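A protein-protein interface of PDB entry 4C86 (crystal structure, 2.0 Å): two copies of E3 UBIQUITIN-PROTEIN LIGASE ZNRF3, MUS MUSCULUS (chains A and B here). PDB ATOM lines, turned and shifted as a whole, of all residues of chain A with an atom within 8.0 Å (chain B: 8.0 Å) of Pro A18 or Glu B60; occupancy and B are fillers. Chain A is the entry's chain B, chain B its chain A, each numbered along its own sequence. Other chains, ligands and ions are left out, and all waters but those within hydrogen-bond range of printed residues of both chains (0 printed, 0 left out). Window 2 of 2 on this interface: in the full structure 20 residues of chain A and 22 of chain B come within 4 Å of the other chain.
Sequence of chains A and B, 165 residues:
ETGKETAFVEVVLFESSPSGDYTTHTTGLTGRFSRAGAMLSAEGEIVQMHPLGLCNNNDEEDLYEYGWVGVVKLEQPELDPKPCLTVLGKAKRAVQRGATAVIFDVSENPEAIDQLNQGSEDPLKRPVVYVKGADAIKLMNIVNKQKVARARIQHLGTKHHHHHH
OH of Tyr B64 sits at hydrogen-bond distance from NH2 of Arg B97, 3.2 Å away.
OG of Ser A19 lies within hydrogen-bond range of OD2 of Asp A21 (2.6 Å).
O of Asp B62 sits at hydrogen-bond distance from NE of Arg B97 (2.9 Å).
The side-chain hydroxyl of Ser A19 sits at hydrogen-bond distance from the side-chain hydroxyl of Ser A17 (2.8 Å).
The side-chain amide oxygen of Asn B58 sits at hydrogen-bond distance from the guanidinium group of Arg B93 (3.1 Å).
ND2 of Asn B57 lies within hydrogen-bond range of OD2 of Asp B59, 3.1 Å away.
ND2 of Asn B58 sits at hydrogen-bond distance from OD1 of Asp A21 (3.0 Å).
The side-chain carboxylate of Glu B60 lies close to the backbone nitrogen of Pro A18 (3.2 Å).
OD1 of Asn B58 sits close to O of Gly A20.
O of Tyr B64 lies within hydrogen-bond range of OH of Tyr A22 (2.8 Å).
The side-chain amide nitrogen (ND2) of Asn B58 is in hydrogen-bond range of the backbone carbonyl oxygen (O) of Ser A19.
No position is printed for both chains.
Of the 15 pairs that touch across the chains among the printed residues, none has its exchanged pair printed and touching as well.
Of chain B, only Glu B60 (3.0 Å) comes within 4 Å of Pro A18.
Printed residues of chain B within 4 Å of Tyr A22: Leu B63, Tyr B64, Glu B65 and Arg B97.
Printed residues of chain B within 4 Å of Ser A16: Glu B60.
The nearest residue of chain B that does not touch Pro A18 is Asn B58 (4.9 Å).
Among the printed residues, merely in contact across the chains: Ser A16 with Glu B60 (3.5 Å), Ser A17 with Glu B60 (3.2 Å), Ser A17 with Leu B63 (3.98 Å), Gly A20 with Asp B59 (3.8 Å), Gly A20 with Glu B60 (3.7 Å), Gly A20 with Leu B63 (3.5 Å), Asp A21 with Leu B63 (3.7 Å), Tyr A22 with Leu B63 (3.7 Å), Tyr A22 with Glu B65 (3.4 Å) and Tyr A22 with Arg B97 (3.5 Å).
Of the 11 printed residues of chain B, 7 touch a printed residue of chain A.
Of the 8 printed residues of chain A, 7 touch a printed residue of chain B.
Hydrophobic or aromatic side chains of chain A within 4 Å of the printed part of chain B: Pro A18 and Tyr A22.
Among the printed residues, 15 pairs touch across the chains.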
ATOM      1  N   GLU A  15      26.171  24.006 -26.718  1.00  0.00           N
ATOM      2  CA  GLU A  15      26.542  25.107 -25.865  1.00  0.00           C
ATOM      3  C   GLU A  15      26.178  24.751 -24.429  1.00  0.00           C
ATOM      4  O   GLU A  15      25.015  24.539 -24.144  1.00  0.00           O
ATOM      5  CB  GLU A  15      25.731  26.316 -26.355  1.00  0.00           C
ATOM      6  CG  GLU A  15      26.239  27.699 -26.024  1.00  0.00           C
ATOM      7  CD  GLU A  15      25.462  28.755 -26.820  1.00  0.00           C
ATOM      8  OE1 GLU A  15      25.794  28.990 -28.008  1.00  0.00           O
ATOM      9  OE2 GLU A  15      24.495  29.333 -26.274  1.00  0.00           O
ATOM     10  N   SER A  16      27.167  24.666 -23.529  1.00  0.00           N
ATOM     11  CA  SER A  16      26.897  24.520 -22.082  1.00  0.00           C
ATOM     12  C   SER A  16      26.184  25.757 -21.589  1.00  0.00           C
ATOM     13  O   SER A  16      26.439  26.845 -22.096  1.00  0.00           O
ATOM     14  CB  SER A  16      28.165  24.391 -21.236  1.00  0.00           C
ATOM     15  OG  SER A  16      29.242  23.869 -21.964  1.00  0.00           O
ATOM     16  N   SER A  17      25.282  25.577 -20.624  1.00  0.00           N
ATOM     17  CA  SER A  17      24.664  26.692 -19.904  1.00  0.00           C
ATOM     18  C   SER A  17      25.045  26.604 -18.422  1.00  0.00           C
ATOM     19  O   SER A  17      25.162  25.495 -17.884  1.00  0.00           O
ATOM     20  CB  SER A  17      23.141  26.662 -20.026  1.00  0.00           C
ATOM     21  OG  SER A  17      22.582  27.863 -19.518  1.00  0.00           O
ATOM     22  N   PRO A  18      25.269  27.767 -17.770  1.00  0.00           N
ATOM     23  CA  PRO A  18      25.386  27.884 -16.293  1.00  0.00           C
ATOM     24  C   PRO A  18      24.179  27.316 -15.570  1.00  0.00           C
ATOM     25  O   PRO A  18      24.286  26.838 -14.432  1.00  0.00           O
ATOM     26  CB  PRO A  18      25.441  29.395 -16.068  1.00  0.00           C
ATOM     27  CG  PRO A  18      26.031  29.944 -17.326  1.00  0.00           C
ATOM     28  CD  PRO A  18      25.560  29.052 -18.446  1.00  0.00           C
ATOM     29  N   SER A  19      23.038  27.384 -16.253  1.00  0.00           N
ATOM     30  CA  SER A  19      21.798  26.792 -15.792  1.00  0.00           C
ATOM     31  C   SER A  19      21.836  25.259 -15.757  1.00  0.00           C
ATOM     32  O   SER A  19      20.861  24.643 -15.380  1.00  0.00           O
ATOM     33  CB  SER A  19      20.654  27.253 -16.706  1.00  0.00           C
ATOM     34  OG  SER A  19      20.683  26.571 -17.945  1.00  0.00           O
ATOM     35  N   GLY A  20      22.941  24.656 -16.187  1.00  0.00           N
ATOM     36  CA  GLY A  20      23.121  23.200 -16.118  1.00  0.00           C
ATOM     37  C   GLY A  20      22.417  22.425 -17.212  1.00  0.00           C
ATOM     38  O   GLY A  20      22.216  21.199 -17.087  1.00  0.00           O
ATOM     39  N   ASP A  21      22.059  23.137 -18.288  1.00  0.00           N
ATOM     40  CA  ASP A  21      21.412  22.534 -19.462  1.00  0.00           C
ATOM     41  C   ASP A  21      22.254  22.713 -20.751  1.00  0.00           C
ATOM     42  O   ASP A  21      22.785  23.794 -21.002  1.00  0.00           O
ATOM     43  CB  ASP A  21      20.015  23.151 -19.629  1.00  0.00           C
ATOM     44  CG  ASP A  21      19.309  23.357 -18.294  1.00  0.00           C
ATOM     45  OD1 ASP A  21      18.972  22.345 -17.624  1.00  0.00           O
ATOM     46  OD2 ASP A  21      19.125  24.535 -17.908  1.00  0.00           O
ATOM     47  N   TYR A  22      22.396  21.651 -21.550  1.00  0.00           N
ATOM     48  CA  TYR A  22      22.934  21.790 -22.919  1.00  0.00           C
ATOM     49  C   TYR A  22      21.855  22.421 -23.812  1.00  0.00           C
ATOM     50  O   TYR A  22      20.671  22.020 -23.778  1.00  0.00           O
ATOM     51  CB  TYR A  22      23.403  20.450 -23.514  1.00  0.00           C
ATOM     52  CG  TYR A  22      24.909  20.194 -23.514  1.00  0.00           C
ATOM     53  CD1 TYR A  22      25.788  21.033 -24.190  1.00  0.00           C
ATOM     54  CD2 TYR A  22      25.443  19.085 -22.893  1.00  0.00           C
ATOM     55  CE1 TYR A  22      27.151  20.792 -24.183  1.00  0.00           C
ATOM     56  CE2 TYR A  22      26.803  18.830 -22.901  1.00  0.00           C
ATOM     57  CZ  TYR A  22      27.650  19.685 -23.549  1.00  0.00           C
ATOM     58  OH  TYR A  22      29.015  19.445 -23.559  1.00  0.00           O
ATOM     59  N   ASN B  57      21.692  17.751  -9.346  1.00  0.00           N
ATOM     60  CA  ASN B  57      21.755  19.122  -8.844  1.00  0.00           C
ATOM     61  C   ASN B  57      21.701  20.123 -10.028  1.00  0.00           C
ATOM     62  O   ASN B  57      21.576  21.335  -9.851  1.00  0.00           O
ATOM     63  CB  ASN B  57      23.040  19.290  -8.045  1.00  0.00           C
ATOM     64  CG  ASN B  57      23.080  20.579  -7.249  1.00  0.00           C
ATOM     65  OD1 ASN B  57      22.173  21.411  -7.332  1.00  0.00           O
ATOM     66  ND2 ASN B  57      24.143  20.749  -6.468  1.00  0.00           N
ATOM     67  N   ASN B  58      21.803  19.587 -11.238  1.00  0.00           N
ATOM     68  CA  ASN B  58      21.733  20.357 -12.484  1.00  0.00           C
ATOM     69  C   ASN B  58      22.828  21.385 -12.668  1.00  0.00           C
ATOM     70  O   ASN B  58      22.580  22.462 -13.149  1.00  0.00           O
ATOM     71  CB  ASN B  58      20.342  20.994 -12.711  1.00  0.00           C
ATOM     72  CG  ASN B  58      19.957  21.027 -14.192  1.00  0.00           C
ATOM     73  OD1 ASN B  58      20.263  20.100 -14.931  1.00  0.00           O
ATOM     74  ND2 ASN B  58      19.327  22.106 -14.634  1.00  0.00           N
ATOM     75  N   ASP B  59      24.056  21.000 -12.388  1.00  0.00           N
ATOM     76  CA  ASP B  59      25.181  21.926 -12.486  1.00  0.00           C
ATOM     77  C   ASP B  59      25.843  21.918 -13.867  1.00  0.00           C
ATOM     78  O   ASP B  59      25.970  20.861 -14.483  1.00  0.00           O
ATOM     79  CB  ASP B  59      26.212  21.558 -11.419  1.00  0.00           C
ATOM     80  CG  ASP B  59      25.743  21.904 -10.011  1.00  0.00           C
ATOM     81  OD1 ASP B  59      25.471  23.095  -9.742  1.00  0.00           O
ATOM     82  OD2 ASP B  59      25.649  20.980  -9.185  1.00  0.00           O
ATOM     83  N   GLU B  60      26.311  23.087 -14.319  1.00  0.00           N
ATOM     84  CA  GLU B  60      27.044  23.206 -15.586  1.00  0.00           C
ATOM     85  C   GLU B  60      28.228  22.243 -15.732  1.00  0.00           C
ATOM     86  O   GLU B  60      28.454  21.683 -16.833  1.00  0.00           O
ATOM     87  CB  GLU B  60      27.555  24.627 -15.812  1.00  0.00           C
ATOM     88  CG  GLU B  60      28.163  24.770 -17.204  1.00  0.00           C
ATOM     89  CD  GLU B  60      28.620  26.160 -17.555  1.00  0.00           C
ATOM     90  OE1 GLU B  60      28.263  27.120 -16.842  1.00  0.00           O
ATOM     91  OE2 GLU B  60      29.346  26.277 -18.566  1.00  0.00           O
ATOM     92  N   GLU B  61      28.985  22.060 -14.643  1.00  0.00           N
ATOM     93  CA  GLU B  61      30.144  21.149 -14.664  1.00  0.00           C
ATOM     94  C   GLU B  61      29.732  19.678 -14.891  1.00  0.00           C
ATOM     95  O   GLU B  61      30.557  18.859 -15.238  1.00  0.00           O
ATOM     96  CB  GLU B  61      30.994  21.258 -13.377  1.00  0.00           C
ATOM     97  CG  GLU B  61      30.267  20.880 -12.085  1.00  0.00           C
ATOM     98  CD  GLU B  61      29.658  22.074 -11.387  1.00  0.00           C
ATOM     99  OE1 GLU B  61      29.361  23.068 -12.074  1.00  0.00           O
ATOM    100  OE2 GLU B  61      29.464  22.019 -10.159  1.00  0.00           O
ATOM    101  N   ASP B  62      28.466  19.342 -14.664  1.00  0.00           N
ATOM    102  CA  ASP B  62      27.989  17.989 -14.996  1.00  0.00           C
ATOM    103  C   ASP B  62      27.818  17.785 -16.519  1.00  0.00           C
ATOM    104  O   ASP B  62      27.665  16.667 -16.970  1.00  0.00           O
ATOM    105  CB  ASP B  62      26.671  17.691 -14.264  1.00  0.00           C
ATOM    106  CG  ASP B  62      26.843  17.648 -12.727  1.00  0.00           C
ATOM    107  OD1 ASP B  62      27.954  17.358 -12.256  1.00  0.00           O
ATOM    108  OD2 ASP B  62      25.869  17.911 -12.001  1.00  0.00           O
ATOM    109  N   LEU B  63      27.848  18.846 -17.318  1.00  0.00           N
ATOM    110  CA  LEU B  63      27.697  18.660 -18.757  1.00  0.00           C
ATOM    111  C   LEU B  63      29.045  18.344 -19.414  1.00  0.00           C
ATOM    112  O   LEU B  63      29.842  19.251 -19.701  1.00  0.00           O
ATOM    113  CB  LEU B  63      27.073  19.900 -19.373  1.00  0.00           C
ATOM    114  CG  LEU B  63      25.815  20.387 -18.683  1.00  0.00           C
ATOM    115  CD1 LEU B  63      25.484  21.762 -19.240  1.00  0.00           C
ATOM    116  CD2 LEU B  63      24.631  19.424 -18.802  1.00  0.00           C
ATOM    117  N   TYR B  64      29.295  17.058 -19.661  1.00  0.00           N
ATOM    118  CA  TYR B  64      30.549  16.616 -20.318  1.00  0.00           C
ATOM    119  C   TYR B  64      30.554  16.943 -21.787  1.00  0.00           C
ATOM    120  O   TYR B  64      29.493  16.930 -22.405  1.00  0.00           O
ATOM    121  CB  TYR B  64      30.772  15.116 -20.123  1.00  0.00           C
ATOM    122  CG  TYR B  64      30.816  14.747 -18.668  1.00  0.00           C
ATOM    123  CD1 TYR B  64      31.350  15.644 -17.715  1.00  0.00           C
ATOM    124  CD2 TYR B  64      30.311  13.537 -18.223  1.00  0.00           C
ATOM    125  CE1 TYR B  64      31.383  15.324 -16.374  1.00  0.00           C
ATOM    126  CE2 TYR B  64      30.349  13.212 -16.879  1.00  0.00           C
ATOM    127  CZ  TYR B  64      30.891  14.101 -15.963  1.00  0.00           C
ATOM    128  OH  TYR B  64      30.925  13.782 -14.625  1.00  0.00           O
ATOM    129  N   GLU B  65      31.744  17.251 -22.321  1.00  0.00           N
ATOM    130  CA  GLU B  65      31.937  17.588 -23.739  1.00  0.00           C
ATOM    131  C   GLU B  65      30.946  16.797 -24.615  1.00  0.00           C
ATOM    132  O   GLU B  65      30.984  15.595 -24.633  1.00  0.00           O
ATOM    133  CB  GLU B  65      33.394  17.300 -24.184  1.00  0.00           C
ATOM    134  CG  GLU B  65      33.646  17.476 -25.692  1.00  0.00           C
ATOM    135  CD  GLU B  65      35.034  17.026 -26.157  1.00  0.00           C
ATOM    136  OE1 GLU B  65      35.999  17.817 -26.040  1.00  0.00           O
ATOM    137  OE2 GLU B  65      35.172  15.886 -26.670  1.00  0.00           O
ATOM    138  N   ARG B  93      19.062  11.373 -17.981  1.00  0.00           N
ATOM    139  CA  ARG B  93      19.815  12.396 -17.379  1.00  0.00           C
ATOM    140  C   ARG B  93      21.150  12.399 -18.099  1.00  0.00           C
ATOM    141  O   ARG B  93      21.603  13.432 -18.516  1.00  0.00           O
ATOM    142  CB  ARG B  93      19.967  12.101 -15.879  1.00  0.00           C
ATOM    143  CG  ARG B  93      20.838  13.123 -15.124  1.00  0.00           C
ATOM    144  CD  ARG B  93      20.266  14.530 -15.185  1.00  0.00           C
ATOM    145  NE  ARG B  93      21.243  15.528 -14.693  1.00  0.00           N
ATOM    146  CZ  ARG B  93      21.352  16.786 -15.130  1.00  0.00           C
ATOM    147  NH1 ARG B  93      20.564  17.260 -16.112  1.00  0.00           N
ATOM    148  NH2 ARG B  93      22.256  17.599 -14.581  1.00  0.00           N
ATOM    149  N   ARG B  97      22.975  15.517 -20.107  1.00  0.00           N
ATOM    150  CA  ARG B  97      24.327  15.931 -19.803  1.00  0.00           C
ATOM    151  C   ARG B  97      25.269  15.802 -20.975  1.00  0.00           C
ATOM    152  O   ARG B  97      26.473  15.978 -20.818  1.00  0.00           O
ATOM    153  CB  ARG B  97      24.823  15.203 -18.577  1.00  0.00           C
ATOM    154  CG  ARG B  97      23.924  15.505 -17.377  1.00  0.00           C
ATOM    155  CD  ARG B  97      24.386  14.824 -16.075  1.00  0.00           C
ATOM    156  NE  ARG B  97      25.826  14.722 -15.950  1.00  0.00           N
ATOM    157  CZ  ARG B  97      26.470  14.091 -14.964  1.00  0.00           C
ATOM    158  NH1 ARG B  97      25.825  13.518 -13.958  1.00  0.00           N
ATOM    159  NH2 ARG B  97      27.790  14.066 -14.982  1.00  0.00           N
